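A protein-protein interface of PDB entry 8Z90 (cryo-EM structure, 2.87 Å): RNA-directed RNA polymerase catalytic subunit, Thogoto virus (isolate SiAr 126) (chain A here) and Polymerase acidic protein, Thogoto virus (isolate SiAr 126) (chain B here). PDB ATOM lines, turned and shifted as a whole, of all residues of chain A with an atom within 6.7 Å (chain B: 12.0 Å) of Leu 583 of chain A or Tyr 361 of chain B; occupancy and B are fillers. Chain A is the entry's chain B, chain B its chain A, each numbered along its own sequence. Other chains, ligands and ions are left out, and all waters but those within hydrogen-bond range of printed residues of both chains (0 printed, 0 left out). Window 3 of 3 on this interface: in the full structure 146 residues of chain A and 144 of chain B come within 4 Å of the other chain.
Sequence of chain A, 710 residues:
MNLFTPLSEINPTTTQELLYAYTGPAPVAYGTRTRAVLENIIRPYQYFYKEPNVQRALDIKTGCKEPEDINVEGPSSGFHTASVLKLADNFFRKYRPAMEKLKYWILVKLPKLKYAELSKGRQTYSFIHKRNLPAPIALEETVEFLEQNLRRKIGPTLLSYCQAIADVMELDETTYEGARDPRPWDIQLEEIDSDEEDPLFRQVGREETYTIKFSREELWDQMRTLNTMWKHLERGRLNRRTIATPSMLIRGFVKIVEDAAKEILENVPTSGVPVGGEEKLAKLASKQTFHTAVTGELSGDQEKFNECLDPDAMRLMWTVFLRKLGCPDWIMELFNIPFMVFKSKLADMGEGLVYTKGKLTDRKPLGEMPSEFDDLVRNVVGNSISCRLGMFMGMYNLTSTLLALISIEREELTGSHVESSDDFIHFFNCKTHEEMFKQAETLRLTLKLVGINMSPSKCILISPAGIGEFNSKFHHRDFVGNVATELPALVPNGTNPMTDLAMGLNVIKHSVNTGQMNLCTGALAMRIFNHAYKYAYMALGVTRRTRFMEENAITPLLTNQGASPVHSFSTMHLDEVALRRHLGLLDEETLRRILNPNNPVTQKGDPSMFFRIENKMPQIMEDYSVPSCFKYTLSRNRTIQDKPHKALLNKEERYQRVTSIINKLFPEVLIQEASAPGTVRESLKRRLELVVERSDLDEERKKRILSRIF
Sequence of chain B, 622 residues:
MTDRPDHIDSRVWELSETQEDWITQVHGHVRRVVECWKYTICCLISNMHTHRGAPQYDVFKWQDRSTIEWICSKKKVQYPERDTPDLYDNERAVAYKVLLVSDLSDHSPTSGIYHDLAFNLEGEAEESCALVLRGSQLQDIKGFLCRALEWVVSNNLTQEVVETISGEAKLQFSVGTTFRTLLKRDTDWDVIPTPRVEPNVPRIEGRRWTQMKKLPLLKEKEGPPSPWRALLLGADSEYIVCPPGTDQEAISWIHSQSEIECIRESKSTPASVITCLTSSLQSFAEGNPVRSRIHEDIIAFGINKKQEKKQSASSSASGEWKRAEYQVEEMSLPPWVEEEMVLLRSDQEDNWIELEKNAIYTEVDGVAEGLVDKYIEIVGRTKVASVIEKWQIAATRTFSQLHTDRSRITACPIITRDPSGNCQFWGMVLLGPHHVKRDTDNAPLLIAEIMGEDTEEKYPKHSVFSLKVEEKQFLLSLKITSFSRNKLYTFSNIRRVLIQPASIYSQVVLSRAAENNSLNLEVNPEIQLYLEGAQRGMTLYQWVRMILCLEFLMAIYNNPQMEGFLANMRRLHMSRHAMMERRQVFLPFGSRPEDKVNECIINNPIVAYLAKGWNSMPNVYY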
ATOM      1  N   PRO A 565      35.455  11.979  -7.618  1.00  0.00           N
ATOM      2  CA  PRO A 565      34.126  12.522  -7.319  1.00  0.00           C
ATOM      3  C   PRO A 565      33.532  11.924  -6.054  1.00  0.00           C
ATOM      4  O   PRO A 565      33.732  10.750  -5.734  1.00  0.00           O
ATOM      5  CB  PRO A 565      33.309  12.134  -8.554  1.00  0.00           C
ATOM      6  CG  PRO A 565      33.954  10.872  -9.010  1.00  0.00           C
ATOM      7  CD  PRO A 565      35.428  11.135  -8.826  1.00  0.00           C
ATOM      8  N   VAL A 566      32.790  12.761  -5.335  1.00  0.00           N
ATOM      9  CA  VAL A 566      32.101  12.334  -4.127  1.00  0.00           C
ATOM     10  C   VAL A 566      30.585  12.333  -4.295  1.00  0.00           C
ATOM     11  O   VAL A 566      29.904  11.551  -3.613  1.00  0.00           O
ATOM     12  CB  VAL A 566      32.511  13.204  -2.919  1.00  0.00           C
ATOM     13  CG1 VAL A 566      32.009  14.632  -3.084  1.00  0.00           C
ATOM     14  CG2 VAL A 566      32.026  12.594  -1.613  1.00  0.00           C
ATOM     15  N   HIS A 567      30.039  13.155  -5.188  1.00  0.00           N
ATOM     16  CA  HIS A 567      28.601  13.196  -5.408  1.00  0.00           C
ATOM     17  C   HIS A 567      28.139  11.967  -6.176  1.00  0.00           C
ATOM     18  O   HIS A 567      28.837  11.467  -7.062  1.00  0.00           O
ATOM     19  CB  HIS A 567      28.213  14.461  -6.172  1.00  0.00           C
ATOM     20  CG  HIS A 567      28.323  15.713  -5.361  1.00  0.00           C
ATOM     21  ND1 HIS A 567      27.409  16.048  -4.385  1.00  0.00           N
ATOM     22  CD2 HIS A 567      29.235  16.711  -5.381  1.00  0.00           C
ATOM     23  CE1 HIS A 567      27.757  17.198  -3.837  1.00  0.00           C
ATOM     24  NE2 HIS A 567      28.862  17.623  -4.424  1.00  0.00           N
ATOM     25  N   SER A 568      26.950  11.484  -5.828  1.00  0.00           N
ATOM     26  CA  SER A 568      26.365  10.330  -6.497  1.00  0.00           C
ATOM     27  C   SER A 568      24.925  10.627  -6.893  1.00  0.00           C
ATOM     28  O   SER A 568      24.447  11.750  -6.705  1.00  0.00           O
ATOM     29  CB  SER A 568      26.436   9.102  -5.594  1.00  0.00           C
ATOM     30  OG  SER A 568      25.642   9.274  -4.435  1.00  0.00           O
ATOM     31  N   PHE A 569      24.226   9.637  -7.452  1.00  0.00           N
ATOM     32  CA  PHE A 569      22.852   9.870  -7.884  1.00  0.00           C
ATOM     33  C   PHE A 569      21.933  10.090  -6.691  1.00  0.00           C
ATOM     34  O   PHE A 569      20.947  10.829  -6.781  1.00  0.00           O
ATOM     35  CB  PHE A 569      22.349   8.709  -8.737  1.00  0.00           C
ATOM     36  CG  PHE A 569      20.964   8.920  -9.267  1.00  0.00           C
ATOM     37  CD1 PHE A 569      20.707   9.948 -10.158  1.00  0.00           C
ATOM     38  CD2 PHE A 569      19.913   8.126  -8.847  1.00  0.00           C
ATOM     39  CE1 PHE A 569      19.435  10.162 -10.643  1.00  0.00           C
ATOM     40  CE2 PHE A 569      18.637   8.341  -9.325  1.00  0.00           C
ATOM     41  CZ  PHE A 569      18.399   9.358 -10.227  1.00  0.00           C
ATOM     42  N   SER A 570      22.219   9.426  -5.572  1.00  0.00           N
ATOM     43  CA  SER A 570      21.454   9.681  -4.357  1.00  0.00           C
ATOM     44  C   SER A 570      21.865  11.002  -3.720  1.00  0.00           C
ATOM     45  O   SER A 570      21.023  11.728  -3.177  1.00  0.00           O
ATOM     46  CB  SER A 570      21.634   8.526  -3.374  1.00  0.00           C
ATOM     47  OG  SER A 570      21.411   7.279  -4.008  1.00  0.00           O
ATOM     48  N   THR A 571      23.154  11.331  -3.775  1.00  0.00           N
ATOM     49  CA  THR A 571      23.683  12.532  -3.127  1.00  0.00           C
ATOM     50  C   THR A 571      23.841  13.678  -4.128  1.00  0.00           C
ATOM     51  O   THR A 571      24.941  14.139  -4.426  1.00  0.00           O
ATOM     52  CB  THR A 571      25.007  12.219  -2.441  1.00  0.00           C
ATOM     53  OG1 THR A 571      26.014  11.980  -3.432  1.00  0.00           O
ATOM     54  CG2 THR A 571      24.871  10.991  -1.563  1.00  0.00           C
ATOM     55  N   ALA A 578      30.188  19.356   2.988  1.00  0.00           N
ATOM     56  CA  ALA A 578      29.622  18.567   4.078  1.00  0.00           C
ATOM     57  C   ALA A 578      29.711  17.074   3.788  1.00  0.00           C
ATOM     58  O   ALA A 578      29.986  16.275   4.692  1.00  0.00           O
ATOM     59  CB  ALA A 578      28.173  18.983   4.328  1.00  0.00           C
ATOM     60  N   LEU A 579      29.476  16.681   2.534  1.00  0.00           N
ATOM     61  CA  LEU A 579      29.580  15.273   2.166  1.00  0.00           C
ATOM     62  C   LEU A 579      30.998  14.755   2.365  1.00  0.00           C
ATOM     63  O   LEU A 579      31.197  13.643   2.865  1.00  0.00           O
ATOM     64  CB  LEU A 579      29.135  15.079   0.717  1.00  0.00           C
ATOM     65  CG  LEU A 579      28.982  13.646   0.210  1.00  0.00           C
ATOM     66  CD1 LEU A 579      28.132  12.831   1.164  1.00  0.00           C
ATOM     67  CD2 LEU A 579      28.382  13.640  -1.185  1.00  0.00           C
ATOM     68  N   ARG A 580      31.998  15.550   1.978  1.00  0.00           N
ATOM     69  CA  ARG A 580      33.385  15.153   2.185  1.00  0.00           C
ATOM     70  C   ARG A 580      33.741  15.111   3.666  1.00  0.00           C
ATOM     71  O   ARG A 580      34.504  14.237   4.092  1.00  0.00           O
ATOM     72  CB  ARG A 580      34.319  16.101   1.435  1.00  0.00           C
ATOM     73  CG  ARG A 580      34.253  15.957  -0.077  1.00  0.00           C
ATOM     74  CD  ARG A 580      35.402  16.676  -0.757  1.00  0.00           C
ATOM     75  NE  ARG A 580      35.308  16.602  -2.209  1.00  0.00           N
ATOM     76  CZ  ARG A 580      35.712  15.570  -2.937  1.00  0.00           C
ATOM     77  NH1 ARG A 580      36.253  14.500  -2.378  1.00  0.00           N
ATOM     78  NH2 ARG A 580      35.572  15.614  -4.259  1.00  0.00           N
ATOM     79  N   ARG A 581      33.210  16.045   4.461  1.00  0.00           N
ATOM     80  CA  ARG A 581      33.460  16.019   5.899  1.00  0.00           C
ATOM     81  C   ARG A 581      32.893  14.756   6.534  1.00  0.00           C
ATOM     82  O   ARG A 581      33.545  14.120   7.370  1.00  0.00           O
ATOM     83  CB  ARG A 581      32.863  17.254   6.570  1.00  0.00           C
ATOM     84  CG  ARG A 581      33.161  17.319   8.061  1.00  0.00           C
ATOM     85  CD  ARG A 581      32.627  18.585   8.705  1.00  0.00           C
ATOM     86  NE  ARG A 581      32.905  18.611  10.136  1.00  0.00           N
ATOM     87  CZ  ARG A 581      32.573  19.605  10.947  1.00  0.00           C
ATOM     88  NH1 ARG A 581      31.942  20.679  10.501  1.00  0.00           N
ATOM     89  NH2 ARG A 581      32.881  19.521  12.238  1.00  0.00           N
ATOM     90  N   HIS A 582      31.670  14.382   6.153  1.00  0.00           N
ATOM     91  CA  HIS A 582      31.027  13.229   6.776  1.00  0.00           C
ATOM     92  C   HIS A 582      31.782  11.940   6.472  1.00  0.00           C
ATOM     93  O   HIS A 582      31.911  11.071   7.342  1.00  0.00           O
ATOM     94  CB  HIS A 582      29.576  13.121   6.314  1.00  0.00           C
ATOM     95  CG  HIS A 582      28.881  11.885   6.794  1.00  0.00           C
ATOM     96  ND1 HIS A 582      28.775  10.746   6.026  1.00  0.00           N
ATOM     97  CD2 HIS A 582      28.259  11.610   7.964  1.00  0.00           C
ATOM     98  CE1 HIS A 582      28.116   9.821   6.703  1.00  0.00           C
ATOM     99  NE2 HIS A 582      27.792  10.321   7.881  1.00  0.00           N
ATOM    100  N   LEU A 583      32.286  11.799   5.248  1.00  0.00           N
ATOM    101  CA  LEU A 583      33.008  10.595   4.859  1.00  0.00           C
ATOM    102  C   LEU A 583      34.483  10.633   5.234  1.00  0.00           C
ATOM    103  O   LEU A 583      35.185   9.639   5.014  1.00  0.00           O
ATOM    104  CB  LEU A 583      32.862  10.364   3.353  1.00  0.00           C
ATOM    105  CG  LEU A 583      31.418  10.312   2.852  1.00  0.00           C
ATOM    106  CD1 LEU A 583      31.355  10.594   1.365  1.00  0.00           C
ATOM    107  CD2 LEU A 583      30.788   8.966   3.171  1.00  0.00           C
ATOM    108  N   GLY A 584      34.969  11.740   5.789  1.00  0.00           N
ATOM    109  CA  GLY A 584      36.348  11.811   6.225  1.00  0.00           C
ATOM    110  C   GLY A 584      37.338  12.256   5.177  1.00  0.00           C
ATOM    111  O   GLY A 584      38.517  11.898   5.264  1.00  0.00           O
ATOM    112  N   LEU A 585      36.902  13.027   4.182  1.00  0.00           N
ATOM    113  CA  LEU A 585      37.795  13.496   3.133  1.00  0.00           C
ATOM    114  C   LEU A 585      38.366  14.880   3.409  1.00  0.00           C
ATOM    115  O   LEU A 585      39.359  15.262   2.780  1.00  0.00           O
ATOM    116  CB  LEU A 585      37.063  13.500   1.787  1.00  0.00           C
ATOM    117  CG  LEU A 585      36.658  12.116   1.273  1.00  0.00           C
ATOM    118  CD1 LEU A 585      35.819  12.229   0.012  1.00  0.00           C
ATOM    119  CD2 LEU A 585      37.885  11.254   1.031  1.00  0.00           C
ATOM    120  N   LEU A 586      37.763  15.634   4.324  1.00  0.00           N
ATOM    121  CA  LEU A 586      38.243  16.952   4.723  1.00  0.00           C
ATOM    122  C   LEU A 586      38.303  16.971   6.243  1.00  0.00           C
ATOM    123  O   LEU A 586      37.304  17.288   6.897  1.00  0.00           O
ATOM    124  CB  LEU A 586      37.311  18.049   4.203  1.00  0.00           C
ATOM    125  CG  LEU A 586      37.487  18.504   2.753  1.00  0.00           C
ATOM    126  CD1 LEU A 586      36.465  19.575   2.405  1.00  0.00           C
ATOM    127  CD2 LEU A 586      38.894  18.994   2.484  1.00  0.00           C
ATOM    128  N   GLU B 356      35.002   8.895 -15.664  1.00  0.00           N
ATOM    129  CA  GLU B 356      35.214   8.506 -14.277  1.00  0.00           C
ATOM    130  C   GLU B 356      33.882   8.182 -13.614  1.00  0.00           C
ATOM    131  O   GLU B 356      32.920   8.947 -13.718  1.00  0.00           O
ATOM    132  CB  GLU B 356      35.929   9.623 -13.518  1.00  0.00           C
ATOM    133  CG  GLU B 356      36.587   9.171 -12.226  1.00  0.00           C
ATOM    134  CD  GLU B 356      37.466  10.243 -11.614  1.00  0.00           C
ATOM    135  OE1 GLU B 356      37.274  11.432 -11.945  1.00  0.00           O
ATOM    136  OE2 GLU B 356      38.352   9.898 -10.805  1.00  0.00           O
ATOM    137  N   LYS B 357      33.830   7.042 -12.933  1.00  0.00           N
ATOM    138  CA  LYS B 357      32.609   6.615 -12.272  1.00  0.00           C
ATOM    139  C   LYS B 357      32.319   7.518 -11.076  1.00  0.00           C
ATOM    140  O   LYS B 357      33.217   8.102 -10.464  1.00  0.00           O
ATOM    141  CB  LYS B 357      32.724   5.158 -11.838  1.00  0.00           C
ATOM    142  CG  LYS B 357      32.823   4.175 -12.987  1.00  0.00           C
ATOM    143  CD  LYS B 357      32.923   2.748 -12.478  1.00  0.00           C
ATOM    144  CE  LYS B 357      32.932   1.757 -13.627  1.00  0.00           C
ATOM    145  NZ  LYS B 357      34.163   1.877 -14.453  1.00  0.00           N
ATOM    146  N   ASN B 358      31.040   7.631 -10.738  1.00  0.00           N
ATOM    147  CA  ASN B 358      30.600   8.377  -9.571  1.00  0.00           C
ATOM    148  C   ASN B 358      30.572   7.447  -8.366  1.00  0.00           C
ATOM    149  O   ASN B 358      30.670   6.224  -8.490  1.00  0.00           O
ATOM    150  CB  ASN B 358      29.220   9.004  -9.798  1.00  0.00           C
ATOM    151  CG  ASN B 358      29.252  10.134 -10.804  1.00  0.00           C
ATOM    152  OD1 ASN B 358      30.306  10.708 -11.079  1.00  0.00           O
ATOM    153  ND2 ASN B 358      28.094  10.457 -11.367  1.00  0.00           N
ATOM    154  N   ALA B 359      30.438   8.045  -7.187  1.00  0.00           N
ATOM    155  CA  ALA B 359      30.411   7.268  -5.960  1.00  0.00           C
ATOM    156  C   ALA B 359      29.135   6.433  -5.881  1.00  0.00           C
ATOM    157  O   ALA B 359      28.150   6.680  -6.581  1.00  0.00           O
ATOM    158  CB  ALA B 359      30.518   8.186  -4.744  1.00  0.00           C
ATOM    159  N   ILE B 360      29.172   5.416  -5.024  1.00  0.00           N
ATOM    160  CA  ILE B 360      28.029   4.546  -4.780  1.00  0.00           C
ATOM    161  C   ILE B 360      27.802   4.482  -3.278  1.00  0.00           C
ATOM    162  O   ILE B 360      28.694   4.064  -2.529  1.00  0.00           O
ATOM    163  CB  ILE B 360      28.236   3.136  -5.358  1.00  0.00           C
ATOM    164  CG1 ILE B 360      28.443   3.205  -6.872  1.00  0.00           C
ATOM    165  CG2 ILE B 360      27.053   2.244  -5.020  1.00  0.00           C
ATOM    166  CD1 ILE B 360      28.652   1.858  -7.521  1.00  0.00           C
ATOM    167  N   TYR B 361      26.616   4.893  -2.838  1.00  0.00           N
ATOM    168  CA  TYR B 361      26.263   4.890  -1.426  1.00  0.00           C
ATOM    169  C   TYR B 361      24.984   4.130  -1.121  1.00  0.00           C
ATOM    170  O   TYR B 361      24.812   3.667   0.008  1.00  0.00           O
ATOM    171  CB  TYR B 361      26.110   6.330  -0.912  1.00  0.00           C
ATOM    172  CG  TYR B 361      27.342   7.183  -1.101  1.00  0.00           C
ATOM    173  CD1 TYR B 361      28.552   6.833  -0.518  1.00  0.00           C
ATOM    174  CD2 TYR B 361      27.293   8.340  -1.864  1.00  0.00           C
ATOM    175  CE1 TYR B 361      29.679   7.612  -0.693  1.00  0.00           C
ATOM    176  CE2 TYR B 361      28.413   9.125  -2.043  1.00  0.00           C
ATOM    177  CZ  TYR B 361      29.603   8.756  -1.456  1.00  0.00           C
ATOM    178  OH  TYR B 361      30.720   9.538  -1.636  1.00  0.00           O
ATOM    179  N   THR B 362      24.090   3.990  -2.091  1.00  0.00           N
ATOM    180  CA  THR B 362      22.792   3.354  -1.919  1.00  0.00           C
ATOM    181  C   THR B 362      22.623   2.299  -3.017  1.00  0.00           C
ATOM    182  O   THR B 362      23.283   2.349  -4.057  1.00  0.00           O
ATOM    183  CB  THR B 362      21.689   4.420  -1.942  1.00  0.00           C
ATOM    184  OG1 THR B 362      21.927   5.368  -0.895  1.00  0.00           O
ATOM    185  CG2 THR B 362      20.310   3.808  -1.730  1.00  0.00           C
ATOM    186  N   GLU B 363      21.750   1.320  -2.770  1.00  0.00           N
ATOM    187  CA  GLU B 363      21.418   0.335  -3.791  1.00  0.00           C
ATOM    188  C   GLU B 363      20.876   0.983  -5.059  1.00  0.00           C
ATOM    189  O   GLU B 363      21.114   0.472  -6.159  1.00  0.00           O
ATOM    190  CB  GLU B 363      20.408  -0.673  -3.234  1.00  0.00           C
ATOM    191  CG  GLU B 363      19.562  -1.384  -4.278  1.00  0.00           C
ATOM    192  CD  GLU B 363      18.576  -2.357  -3.664  1.00  0.00           C
ATOM    193  OE1 GLU B 363      18.442  -3.481  -4.191  1.00  0.00           O
ATOM    194  OE2 GLU B 363      17.934  -1.999  -2.653  1.00  0.00           O
ATOM    195  N   VAL B 364      20.172   2.111  -4.927  1.00  0.00           N
ATOM    196  CA  VAL B 364      19.752   2.874  -6.097  1.00  0.00           C
ATOM    197  C   VAL B 364      20.968   3.352  -6.882  1.00  0.00           C
ATOM    198  O   VAL B 364      20.963   3.367  -8.119  1.00  0.00           O
ATOM    199  CB  VAL B 364      18.863   4.057  -5.671  1.00  0.00           C
ATOM    200  CG1 VAL B 364      18.476   4.903  -6.875  1.00  0.00           C
ATOM    201  CG2 VAL B 364      17.634   3.571  -4.919  1.00  0.00           C
ATOM    202  N   ASP B 365      22.026   3.747  -6.172  1.00  0.00           N
ATOM    203  CA  ASP B 365      23.217   4.282  -6.825  1.00  0.00           C
ATOM    204  C   ASP B 365      23.878   3.237  -7.715  1.00  0.00           C
ATOM    205  O   ASP B 365      24.305   3.545  -8.834  1.00  0.00           O
ATOM    206  CB  ASP B 365      24.196   4.781  -5.765  1.00  0.00           C
ATOM    207  CG  ASP B 365      24.006   6.243  -5.438  1.00  0.00           C
ATOM    208  OD1 ASP B 365      23.068   6.861  -5.981  1.00  0.00           O
ATOM    209  OD2 ASP B 365      24.773   6.763  -4.605  1.00  0.00           O
ATOM    210  N   GLY B 366      23.978   1.997  -7.232  1.00  0.00           N
ATOM    211  CA  GLY B 366      24.582   0.947  -8.035  1.00  0.00           C
ATOM    212  C   GLY B 366      23.767   0.610  -9.268  1.00  0.00           C
ATOM    213  O   GLY B 366      24.324   0.303 -10.325  1.00  0.00           O
ATOM    214  N   VAL B 367      22.439   0.650  -9.147  1.00  0.00           N
ATOM    215  CA  VAL B 367      21.576   0.404 -10.299  1.00  0.00           C
ATOM    216  C   VAL B 367      21.792   1.472 -11.362  1.00  0.00           C
ATOM    217  O   VAL B 367      21.870   1.172 -12.560  1.00  0.00           O
ATOM    218  CB  VAL B 367      20.103   0.334  -9.857  1.00  0.00           C
ATOM    219  CG1 VAL B 367      19.189   0.287 -11.068  1.00  0.00           C
ATOM    220  CG2 VAL B 367      19.876  -0.875  -8.966  1.00  0.00           C
ATOM    221  N   ALA B 368      21.889   2.736 -10.943  1.00  0.00           N
ATOM    222  CA  ALA B 368      22.105   3.818 -11.896  1.00  0.00           C
ATOM    223  C   ALA B 368      23.438   3.663 -12.616  1.00  0.00           C
ATOM    224  O   ALA B 368      23.528   3.899 -13.825  1.00  0.00           O
ATOM    225  CB  ALA B 368      22.034   5.168 -11.181  1.00  0.00           C
ATOM    226  N   GLU B 369      24.480   3.263 -11.894  1.00  0.00           N
ATOM    227  CA  GLU B 369      25.806   3.104 -12.475  1.00  0.00           C
ATOM    228  C   GLU B 369      25.974   1.792 -13.230  1.00  0.00           C
ATOM    229  O   GLU B 369      26.988   1.616 -13.912  1.00  0.00           O
ATOM    230  CB  GLU B 369      26.876   3.215 -11.386  1.00  0.00           C
ATOM    231  CG  GLU B 369      26.946   4.590 -10.750  1.00  0.00           C
ATOM    232  CD  GLU B 369      27.671   5.595 -11.622  1.00  0.00           C
ATOM    233  OE1 GLU B 369      28.292   5.182 -12.624  1.00  0.00           O
ATOM    234  OE2 GLU B 369      27.605   6.802 -11.316  1.00  0.00           O
ATOM    235  N   GLY B 370      25.020   0.873 -13.125  1.00  0.00           N
ATOM    236  CA  GLY B 370      25.063  -0.338 -13.921  1.00  0.00           C
ATOM    237  C   GLY B 370      24.532  -0.089 -15.317  1.00  0.00           C
ATOM    238  O   GLY B 370      25.107  -0.552 -16.308  1.00  0.00           O
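O of Val 566 of chain A is in hydrogen-bond range of OH of Tyr 361 of chain B, at 2.9 Å. The side-chain carboxylate of Asp 365 of chain B sits at hydrogen-bond distance from the side-chain hydroxyl of Ser 570 of chain A (2.6 Å). The side-chain carboxylate of Asp 365 of chain B is in hydrogen-bond range of the side-chain hydroxyl of Ser 568 of chain A, 2.7 Å away. The side-chain carboxylate (OD1) of Asp 365 of chain B is in hydrogen-bond range of the backbone NH (N) of Phe 569 of chain A (3.3 Å).
N of Tyr 361 of chain B sits at hydrogen-bond distance from OD2 of Asp 365 of chain B. The backbone NH (N) of Ser 568 of chain A is in hydrogen-bond range of the side-chain hydroxyl (OG1) of Thr 571 of chain A, at 2.6 Å. A ring nitrogen (ND1) of His 567 of chain A lies within hydrogen-bond range of the backbone carbonyl oxygen (O) of Thr 571 of chain A.
Pro 565 of chain A touches Glu 356 of chain B (CD to CD, 3.6 Å). Pro 565 of chain A touches Lys 357 of chain B (CG to O, 3.2 Å). Ala 359 of chain B touches Val 566 of chain A (CB to O, 3.6 Å). CB of Asn 358 of chain B touches O of His 567 of chain A (3.7 Å). His 567 of chain A touches Ala 359 of chain B (O to N, 3.8 Å). Ser 568 of chain A touches Ala 359 of chain B (CB to O, 3.1 Å). Ser 568 of chain A touches Tyr 361 of chain B (OG to CD2, 3.2 Å). Thr 362 of chain B touches Ser 570 of chain A. CG2 of Thr 571 of chain A touches CD2 of Tyr 361 of chain B (3.6 Å). CD1 of Leu 583 of chain A touches OH of Tyr 361 of chain B, at 3.2 Å.
Leu 583 of chain A touches just one residue of chain B: Tyr 361 (3.2 Å). Tyr 361 of chain B touches just these residues of chain A: Val 566 (2.9 Å), Ser 568 (3.2 Å), Thr 571 (3.6 Å) and Leu 583 (3.2 Å). Val 566 of chain A touches just these residues of chain B: Ala 359 (3.6 Å) and Tyr 361 (2.9 Å). Of chain B, only Thr 362 and Asp 365 come within 4 Å of Ser 570 of chain A. Thr 571 of chain A touches one residue of chain B. No residue of chain B comes within 4 Å of Leu 579 of chain A. No residue of chain B comes within 4 Å of His 582 of chain A. No residue of chain B comes within 4 Å of Gly 584 of chain A. No residue of chain B comes within 4 Å of Leu 585 of chain A. Of the printed residues of chain A, Lys 357 of chain B touches Pro 565. Of the printed residues of chain A, Thr 362 of chain B touches Ser 570. Ile 360 of chain B touches none of the printed residues of chain A. Leu 586 of chain A touches none of the printed residues of chain B. The nearest residue of chain B that does not touch Leu 583 of chain A is Ala 359 of chain B (6.6 Å). The nearest printed residue of chain A that does not touch Ala 359 of chain B is Pro 565 of chain A (4.2 Å).
Printed residues of chain B that touch a printed residue of chain A: Glu 356, Lys 357, Asn 358, Ala 359, Tyr 361, Thr 362 and Asp 365. Hydrophobic or aromatic side chains of chain B that line the printed part of chain A: Ala 359 and Tyr 361. Of the 16 printed residues of chain A, 8 touch a printed residue of chain B. Among the printed residues, 14 pairs touch across the chains. Among the printed residues, no Asp or Glu carboxylate lies within 4 Å of a Lys or Arg side-chain nitrogen of the other chain.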
